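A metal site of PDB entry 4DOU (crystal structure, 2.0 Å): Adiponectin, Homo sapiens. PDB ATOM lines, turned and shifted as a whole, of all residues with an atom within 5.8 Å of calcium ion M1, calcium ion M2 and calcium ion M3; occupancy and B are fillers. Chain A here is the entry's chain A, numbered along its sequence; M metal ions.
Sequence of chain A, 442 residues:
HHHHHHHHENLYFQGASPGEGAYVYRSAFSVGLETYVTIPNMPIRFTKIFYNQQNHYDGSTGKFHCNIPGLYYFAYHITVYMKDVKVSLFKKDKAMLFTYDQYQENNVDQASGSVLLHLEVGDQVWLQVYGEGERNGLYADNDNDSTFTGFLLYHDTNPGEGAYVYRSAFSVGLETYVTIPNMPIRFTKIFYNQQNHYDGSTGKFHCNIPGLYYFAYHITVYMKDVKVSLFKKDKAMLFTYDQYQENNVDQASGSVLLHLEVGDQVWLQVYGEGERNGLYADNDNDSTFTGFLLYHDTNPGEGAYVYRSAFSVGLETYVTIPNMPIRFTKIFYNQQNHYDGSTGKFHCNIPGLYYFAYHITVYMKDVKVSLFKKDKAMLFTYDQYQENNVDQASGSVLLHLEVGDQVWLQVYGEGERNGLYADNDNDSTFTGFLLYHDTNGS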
ATOM      1  N   ASP A 101      -8.035  -0.297 -19.146  1.00  0.00           N
ATOM      2  CA  ASP A 101      -7.916  -0.287 -20.586  1.00  0.00           C
ATOM      3  C   ASP A 101      -8.719  -1.476 -21.125  1.00  0.00           C
ATOM      4  O   ASP A 101      -8.436  -2.623 -20.803  1.00  0.00           O
ATOM      5  CB  ASP A 101      -6.440  -0.387 -20.999  1.00  0.00           C
ATOM      6  CG  ASP A 101      -6.176   0.043 -22.441  1.00  0.00           C
ATOM      7  OD1 ASP A 101      -5.011   0.366 -22.760  1.00  0.00           O
ATOM      8  OD2 ASP A 101      -7.123   0.038 -23.253  1.00  0.00           O
ATOM      9  N   GLN A 102      -9.756  -1.176 -21.911  1.00  0.00           N
ATOM     10  CA  GLN A 102     -10.615  -2.223 -22.467  1.00  0.00           C
ATOM     11  C   GLN A 102      -9.960  -2.813 -23.711  1.00  0.00           C
ATOM     12  O   GLN A 102      -9.235  -2.117 -24.430  1.00  0.00           O
ATOM     13  CB  GLN A 102     -12.009  -1.667 -22.822  1.00  0.00           C
ATOM     14  CG  GLN A 102     -13.001  -1.715 -21.670  1.00  0.00           C
ATOM     15  CD  GLN A 102     -14.345  -1.083 -22.006  1.00  0.00           C
ATOM     16  OE1 GLN A 102     -14.409  -0.005 -22.605  1.00  0.00           O
ATOM     17  NE2 GLN A 102     -15.422  -1.742 -21.613  1.00  0.00           N
ATOM     18  N   TYR A 103     -10.195  -4.098 -23.950  1.00  0.00           N
ATOM     19  CA  TYR A 103      -9.671  -4.786 -25.116  1.00  0.00           C
ATOM     20  C   TYR A 103     -10.781  -5.096 -26.120  1.00  0.00           C
ATOM     21  O   TYR A 103     -11.857  -5.563 -25.757  1.00  0.00           O
ATOM     22  CB  TYR A 103      -8.996  -6.104 -24.731  1.00  0.00           C
ATOM     23  CG  TYR A 103      -8.536  -6.901 -25.937  1.00  0.00           C
ATOM     24  CD1 TYR A 103      -7.407  -6.527 -26.632  1.00  0.00           C
ATOM     25  CD2 TYR A 103      -9.254  -8.000 -26.379  1.00  0.00           C
ATOM     26  CE1 TYR A 103      -6.988  -7.239 -27.749  1.00  0.00           C
ATOM     27  CE2 TYR A 103      -8.844  -8.716 -27.495  1.00  0.00           C
ATOM     28  CZ  TYR A 103      -7.707  -8.330 -28.170  1.00  0.00           C
ATOM     29  OH  TYR A 103      -7.289  -9.033 -29.276  1.00  0.00           O
ATOM     30  N   ASN A 107      -7.320  -5.940 -31.550  1.00  0.00           N
ATOM     31  CA  ASN A 107      -6.887  -4.592 -31.227  1.00  0.00           C
ATOM     32  C   ASN A 107      -6.029  -4.484 -29.958  1.00  0.00           C
ATOM     33  O   ASN A 107      -6.448  -3.908 -28.959  1.00  0.00           O
ATOM     34  CB  ASN A 107      -8.095  -3.673 -31.138  1.00  0.00           C
ATOM     35  CG  ASN A 107      -7.709  -2.218 -31.248  1.00  0.00           C
ATOM     36  OD1 ASN A 107      -6.571  -1.858 -30.989  1.00  0.00           O
ATOM     37  ND2 ASN A 107      -8.659  -1.380 -31.642  1.00  0.00           N
ATOM     38  N   VAL A 108      -4.822  -5.019 -30.016  1.00  0.00           N
ATOM     39  CA  VAL A 108      -3.891  -4.918 -28.905  1.00  0.00           C
ATOM     40  C   VAL A 108      -3.694  -3.460 -28.493  1.00  0.00           C
ATOM     41  O   VAL A 108      -3.489  -2.573 -29.340  1.00  0.00           O
ATOM     42  CB  VAL A 108      -2.540  -5.553 -29.255  1.00  0.00           C
ATOM     43  CG1 VAL A 108      -1.521  -5.331 -28.156  1.00  0.00           C
ATOM     44  CG2 VAL A 108      -2.736  -7.052 -29.558  1.00  0.00           C
ATOM     45  N   ASP A 109      -3.750  -3.231 -27.177  1.00  0.00           N
ATOM     46  CA  ASP A 109      -3.598  -1.893 -26.605  1.00  0.00           C
ATOM     47  C   ASP A 109      -2.398  -1.728 -25.679  1.00  0.00           C
ATOM     48  O   ASP A 109      -1.732  -2.703 -25.294  1.00  0.00           O
ATOM     49  CB  ASP A 109      -4.875  -1.467 -25.882  1.00  0.00           C
ATOM     50  CG  ASP A 109      -5.885  -0.892 -26.838  1.00  0.00           C
ATOM     51  OD1 ASP A 109      -5.481  -0.562 -27.967  1.00  0.00           O
ATOM     52  OD2 ASP A 109      -7.078  -0.767 -26.471  1.00  0.00           O
ATOM     53  N   GLN A 110      -2.119  -0.482 -25.316  1.00  0.00           N
ATOM     54  CA  GLN A 110      -1.047  -0.175 -24.399  1.00  0.00           C
ATOM     55  C   GLN A 110      -1.562   0.709 -23.294  1.00  0.00           C
ATOM     56  O   GLN A 110      -2.053   1.799 -23.558  1.00  0.00           O
ATOM     57  CB  GLN A 110       0.123   0.506 -25.112  1.00  0.00           C
ATOM     58  CG  GLN A 110       0.930  -0.414 -25.997  1.00  0.00           C
ATOM     59  CD  GLN A 110       1.684  -1.469 -25.213  1.00  0.00           C
ATOM     60  OE1 GLN A 110       1.841  -2.620 -25.664  1.00  0.00           O
ATOM     61  NE2 GLN A 110       2.186  -1.082 -24.044  1.00  0.00           N
ATOM     62  N   ASP A 242      -5.880  10.764 -28.598  1.00  0.00           N
ATOM     63  CA  ASP A 242      -6.283   9.376 -28.462  1.00  0.00           C
ATOM     64  C   ASP A 242      -7.760   9.245 -28.786  1.00  0.00           C
ATOM     65  O   ASP A 242      -8.614   9.822 -28.107  1.00  0.00           O
ATOM     66  CB  ASP A 242      -5.965   8.850 -27.053  1.00  0.00           C
ATOM     67  CG  ASP A 242      -5.974   7.322 -26.975  1.00  0.00           C
ATOM     68  OD1 ASP A 242      -6.558   6.690 -27.877  1.00  0.00           O
ATOM     69  OD2 ASP A 242      -5.393   6.745 -26.017  1.00  0.00           O
ATOM     70  N   GLN A 243      -8.061   8.478 -29.825  1.00  0.00           N
ATOM     71  CA  GLN A 243      -9.420   8.356 -30.341  1.00  0.00           C
ATOM     72  C   GLN A 243     -10.219   7.339 -29.553  1.00  0.00           C
ATOM     73  O   GLN A 243      -9.699   6.289 -29.168  1.00  0.00           O
ATOM     74  CB  GLN A 243      -9.403   7.940 -31.815  1.00  0.00           C
ATOM     75  CG  GLN A 243      -9.852   9.009 -32.789  1.00  0.00           C
ATOM     76  CD  GLN A 243     -10.021   8.459 -34.201  1.00  0.00           C
ATOM     77  OE1 GLN A 243      -9.131   7.807 -34.737  1.00  0.00           O
ATOM     78  NE2 GLN A 243     -11.171   8.732 -34.807  1.00  0.00           N
ATOM     79  N   TYR A 244     -11.497   7.630 -29.340  1.00  0.00           N
ATOM     80  CA  TYR A 244     -12.369   6.733 -28.618  1.00  0.00           C
ATOM     81  C   TYR A 244     -13.401   6.060 -29.509  1.00  0.00           C
ATOM     82  O   TYR A 244     -14.211   6.720 -30.148  1.00  0.00           O
ATOM     83  CB  TYR A 244     -13.099   7.467 -27.490  1.00  0.00           C
ATOM     84  CG  TYR A 244     -14.063   6.563 -26.759  1.00  0.00           C
ATOM     85  CD1 TYR A 244     -13.602   5.696 -25.775  1.00  0.00           C
ATOM     86  CD2 TYR A 244     -15.418   6.559 -27.048  1.00  0.00           C
ATOM     87  CE1 TYR A 244     -14.447   4.865 -25.113  1.00  0.00           C
ATOM     88  CE2 TYR A 244     -16.291   5.719 -26.384  1.00  0.00           C
ATOM     89  CZ  TYR A 244     -15.796   4.874 -25.412  1.00  0.00           C
ATOM     90  OH  TYR A 244     -16.614   4.028 -24.733  1.00  0.00           O
ATOM     91  N   GLN A 245     -13.365   4.733 -29.535  1.00  0.00           N
ATOM     92  CA  GLN A 245     -14.424   3.978 -30.175  1.00  0.00           C
ATOM     93  C   GLN A 245     -15.306   3.382 -29.084  1.00  0.00           C
ATOM     94  O   GLN A 245     -14.855   3.170 -27.953  1.00  0.00           O
ATOM     95  CB  GLN A 245     -13.872   2.889 -31.074  1.00  0.00           C
ATOM     96  CG  GLN A 245     -14.752   2.624 -32.300  1.00  0.00           C
ATOM     97  CD  GLN A 245     -14.471   3.599 -33.432  1.00  0.00           C
ATOM     98  OE1 GLN A 245     -15.359   4.324 -33.878  1.00  0.00           O
ATOM     99  NE2 GLN A 245     -13.227   3.622 -33.896  1.00  0.00           N
ATOM    100  N   ASN A 248     -14.645   0.864 -25.936  1.00  0.00           N
ATOM    101  CA  ASN A 248     -13.197   0.691 -25.947  1.00  0.00           C
ATOM    102  C   ASN A 248     -12.459   1.778 -25.176  1.00  0.00           C
ATOM    103  O   ASN A 248     -11.792   2.625 -25.780  1.00  0.00           O
ATOM    104  CB  ASN A 248     -12.670   0.603 -27.383  1.00  0.00           C
ATOM    105  CG  ASN A 248     -11.257   0.046 -27.453  1.00  0.00           C
ATOM    106  OD1 ASN A 248     -10.628  -0.228 -26.433  1.00  0.00           O
ATOM    107  ND2 ASN A 248     -10.741  -0.116 -28.670  1.00  0.00           N
ATOM    108  N   VAL A 249     -12.588   1.765 -23.856  1.00  0.00           N
ATOM    109  CA  VAL A 249     -11.848   2.691 -23.023  1.00  0.00           C
ATOM    110  C   VAL A 249     -10.370   2.501 -23.361  1.00  0.00           C
ATOM    111  O   VAL A 249      -9.886   1.383 -23.540  1.00  0.00           O
ATOM    112  CB  VAL A 249     -12.062   2.426 -21.507  1.00  0.00           C
ATOM    113  CG1 VAL A 249     -11.039   3.216 -20.669  1.00  0.00           C
ATOM    114  CG2 VAL A 249     -13.501   2.755 -21.075  1.00  0.00           C
ATOM    115  N   ASP A 250      -9.664   3.623 -23.480  1.00  0.00           N
ATOM    116  CA  ASP A 250      -8.251   3.604 -23.843  1.00  0.00           C
ATOM    117  C   ASP A 250      -7.423   4.338 -22.787  1.00  0.00           C
ATOM    118  O   ASP A 250      -7.979   4.964 -21.863  1.00  0.00           O
ATOM    119  CB  ASP A 250      -8.042   4.264 -25.226  1.00  0.00           C
ATOM    120  CG  ASP A 250      -8.247   3.285 -26.386  1.00  0.00           C
ATOM    121  OD1 ASP A 250      -8.491   3.738 -27.535  1.00  0.00           O
ATOM    122  OD2 ASP A 250      -8.159   2.058 -26.180  1.00  0.00           O
ATOM    123  N   GLN A 251      -6.108   4.252 -22.932  1.00  0.00           N
ATOM    124  CA  GLN A 251      -5.175   4.938 -22.051  1.00  0.00           C
ATOM    125  C   GLN A 251      -4.153   5.699 -22.866  1.00  0.00           C
ATOM    126  O   GLN A 251      -3.538   5.154 -23.782  1.00  0.00           O
ATOM    127  CB  GLN A 251      -4.454   3.916 -21.162  1.00  0.00           C
ATOM    128  CG  GLN A 251      -5.340   3.290 -20.102  1.00  0.00           C
ATOM    129  CD  GLN A 251      -5.711   4.249 -19.007  1.00  0.00           C
ATOM    130  OE1 GLN A 251      -6.669   4.016 -18.261  1.00  0.00           O
ATOM    131  NE2 GLN A 251      -4.932   5.340 -18.873  1.00  0.00           N
ATOM    132  N   VAL A 362      -0.229   6.194 -32.606  1.00  0.00           N
ATOM    133  CA  VAL A 362      -0.423   5.024 -33.456  1.00  0.00           C
ATOM    134  C   VAL A 362      -1.512   5.328 -34.469  1.00  0.00           C
ATOM    135  O   VAL A 362      -2.682   5.441 -34.116  1.00  0.00           O
ATOM    136  CB  VAL A 362      -0.811   3.810 -32.608  1.00  0.00           C
ATOM    137  CG1 VAL A 362      -0.948   2.545 -33.489  1.00  0.00           C
ATOM    138  CG2 VAL A 362       0.204   3.610 -31.472  1.00  0.00           C
ATOM    139  N   ASP A 383       1.396  -2.181 -30.466  1.00  0.00           N
ATOM    140  CA  ASP A 383       0.080  -1.556 -30.373  1.00  0.00           C
ATOM    141  C   ASP A 383      -0.652  -1.619 -31.723  1.00  0.00           C
ATOM    142  O   ASP A 383      -0.284  -0.957 -32.689  1.00  0.00           O
ATOM    143  CB  ASP A 383       0.196  -0.111 -29.832  1.00  0.00           C
ATOM    144  CG  ASP A 383      -1.135   0.433 -29.329  1.00  0.00           C
ATOM    145  OD1 ASP A 383      -2.184  -0.192 -29.611  1.00  0.00           O
ATOM    146  OD2 ASP A 383      -1.127   1.487 -28.638  1.00  0.00           O
ATOM    147  N   GLN A 384      -1.693  -2.449 -31.776  1.00  0.00           N
ATOM    148  CA  GLN A 384      -2.448  -2.613 -33.018  1.00  0.00           C
ATOM    149  C   GLN A 384      -3.256  -1.369 -33.373  1.00  0.00           C
ATOM    150  O   GLN A 384      -3.641  -0.594 -32.498  1.00  0.00           O
ATOM    151  CB  GLN A 384      -3.357  -3.834 -32.924  1.00  0.00           C
ATOM    152  CG  GLN A 384      -2.704  -5.106 -33.410  1.00  0.00           C
ATOM    153  CD  GLN A 384      -3.665  -6.268 -33.469  1.00  0.00           C
ATOM    154  OE1 GLN A 384      -4.237  -6.661 -32.448  1.00  0.00           O
ATOM    155  NE2 GLN A 384      -3.843  -6.828 -34.660  1.00  0.00           N
ATOM    156  N   TYR A 385      -3.486  -1.171 -34.668  1.00  0.00           N
ATOM    157  CA  TYR A 385      -4.289  -0.034 -35.110  1.00  0.00           C
ATOM    158  C   TYR A 385      -5.585  -0.526 -35.734  1.00  0.00           C
ATOM    159  O   TYR A 385      -5.569  -1.424 -36.579  1.00  0.00           O
ATOM    160  CB  TYR A 385      -3.528   0.843 -36.114  1.00  0.00           C
ATOM    161  CG  TYR A 385      -4.381   1.975 -36.662  1.00  0.00           C
ATOM    162  CD1 TYR A 385      -4.564   3.147 -35.936  1.00  0.00           C
ATOM    163  CD2 TYR A 385      -5.017   1.868 -37.904  1.00  0.00           C
ATOM    164  CE1 TYR A 385      -5.350   4.178 -36.426  1.00  0.00           C
ATOM    165  CE2 TYR A 385      -5.803   2.900 -38.403  1.00  0.00           C
ATOM    166  CZ  TYR A 385      -5.966   4.045 -37.651  1.00  0.00           C
ATOM    167  OH  TYR A 385      -6.741   5.079 -38.131  1.00  0.00           O
ATOM    168  N   GLN A 386      -6.690   0.049 -35.291  1.00  0.00           N
ATOM    169  CA  GLN A 386      -7.987  -0.201 -35.921  1.00  0.00           C
ATOM    170  C   GLN A 386      -8.486   1.078 -36.597  1.00  0.00           C
ATOM    171  O   GLN A 386      -8.336   2.176 -36.049  1.00  0.00           O
ATOM    172  CB  GLN A 386      -9.001  -0.726 -34.903  1.00  0.00           C
ATOM    173  CG  GLN A 386     -10.313  -1.194 -35.504  1.00  0.00           C
ATOM    174  CD  GLN A 386     -11.169  -2.012 -34.538  1.00  0.00           C
ATOM    175  OE1 GLN A 386     -10.740  -2.324 -33.420  1.00  0.00           O
ATOM    176  NE2 GLN A 386     -12.387  -2.361 -34.960  1.00  0.00           N
ATOM    177  N   ASN A 389      -9.349   4.724 -35.206  1.00  0.00           N
ATOM    178  CA  ASN A 389      -8.994   4.595 -33.789  1.00  0.00           C
ATOM    179  C   ASN A 389      -7.518   4.847 -33.528  1.00  0.00           C
ATOM    180  O   ASN A 389      -6.781   3.922 -33.229  1.00  0.00           O
ATOM    181  CB  ASN A 389      -9.410   3.221 -33.239  1.00  0.00           C
ATOM    182  CG  ASN A 389      -9.407   3.177 -31.712  1.00  0.00           C
ATOM    183  OD1 ASN A 389      -8.844   4.053 -31.045  1.00  0.00           O
ATOM    184  ND2 ASN A 389     -10.032   2.147 -31.153  1.00  0.00           N
ATOM    185  N   VAL A 390      -7.095   6.104 -33.653  1.00  0.00           N
ATOM    186  CA  VAL A 390      -5.753   6.492 -33.241  1.00  0.00           C
ATOM    187  C   VAL A 390      -5.531   5.978 -31.822  1.00  0.00           C
ATOM    188  O   VAL A 390      -6.444   6.032 -30.984  1.00  0.00           O
ATOM    189  CB  VAL A 390      -5.570   8.014 -33.267  1.00  0.00           C
ATOM    190  CG1 VAL A 390      -4.313   8.430 -32.503  1.00  0.00           C
ATOM    191  CG2 VAL A 390      -5.528   8.515 -34.713  1.00  0.00           C
ATOM    192  N   ASP A 391      -4.329   5.477 -31.556  1.00  0.00           N
ATOM    193  CA  ASP A 391      -3.937   4.960 -30.244  1.00  0.00           C
ATOM    194  C   ASP A 391      -2.653   5.603 -29.722  1.00  0.00           C
ATOM    195  O   ASP A 391      -1.889   6.230 -30.468  1.00  0.00           O
ATOM    196  CB  ASP A 391      -3.761   3.446 -30.293  1.00  0.00           C
ATOM    197  CG  ASP A 391      -5.040   2.687 -30.047  1.00  0.00           C
ATOM    198  OD1 ASP A 391      -6.017   3.322 -29.614  1.00  0.00           O
ATOM    199  OD2 ASP A 391      -5.071   1.461 -30.262  1.00  0.00           O
ATOM    200  N   GLN A 392      -2.414   5.409 -28.428  1.00  0.00           N
ATOM    201  CA  GLN A 392      -1.220   5.899 -27.774  1.00  0.00           C
ATOM    202  C   GLN A 392      -0.506   4.746 -27.083  1.00  0.00           C
ATOM    203  O   GLN A 392      -1.079   4.072 -26.217  1.00  0.00           O
ATOM    204  CB  GLN A 392      -1.565   6.965 -26.736  1.00  0.00           C
ATOM    205  CG  GLN A 392      -1.960   8.301 -27.339  1.00  0.00           C
ATOM    206  CD  GLN A 392      -0.813   9.027 -28.037  1.00  0.00           C
ATOM    207  OE1 GLN A 392       0.363   8.877 -27.678  1.00  0.00           O
ATOM    208  NE2 GLN A 392      -1.163   9.834 -29.035  1.00  0.00           N
HETATM  209 CA    CA M   1      -8.627   0.181 -25.069  1.00  0.00          CA
HETATM  210 CA    CA M   2      -7.628   5.132 -29.215  1.00  0.00          CA
HETATM  211 CA    CA M   3      -4.395  -0.659 -30.173  1.00  0.00          CA
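Calcium ion M1 is bound by OD2 of Asp 250 (2.2 Å), OD2 of Asp 109 (2.3 Å), O of Val 249 (2.3 Å), OD2 of Asp 101 (2.4 Å), OD1 of Asn 248 (2.5 Å) and O of Gln 102 (2.5 Å). Calcium ion M1 has six donor atoms within binding distance.
Six residues have an atom within 4 Å of calcium ion M2: Asp 242, Gln 243, Asp 250, Asn 389, Val 390 and Asp 391.
Of the 24 residues printed, 6 come within 4 Å of calcium ion M3.
Within 4 Å of calcium ion M1: Asp 101, Gln 102, Asp 109, Asn 248, Val 249 and Asp 250.
Calcium ion M3 is bound by the side-chain carboxylate of Asp 391 (2.2 Å), the backbone carbonyl oxygen of Val 108 (2.3 Å), the side-chain carboxylate of Asp 383 (2.3 Å), the backbone carbonyl oxygen of Gln 384 (2.4 Å), the side-chain carboxylate of Asp 109 (2.5 Å) and the side-chain amide oxygen of Asn 107 (2.6 Å).
Calcium ion M2 is bound by the backbone carbonyl oxygen (O) of Val 390 (2.3 Å), the side-chain carboxylate (OD1) of Asp 242 (2.3 Å), the side-chain carboxylate (OD1) of Asp 250 (2.3 Å), the backbone carbonyl oxygen (O) of Gln 243 (2.4 Å), the side-chain amide oxygen (OD1) of Asn 389 (2.4 Å) and the side-chain carboxylate (OD1) of Asp 391 (2.5 Å).
The backbone carbonyl oxygen (O) of Asp 391 sits at hydrogen-bond distance from the backbone NH (N) of Val 362. ND2 of Asn 389 lies close to ND2 of Asn 248 (3.4 Å). The side-chain amide nitrogen (ND2) of Asn 107 sits at hydrogen-bond distance from the side-chain amide oxygen (OE1) of Gln 386, at 2.9 Å.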
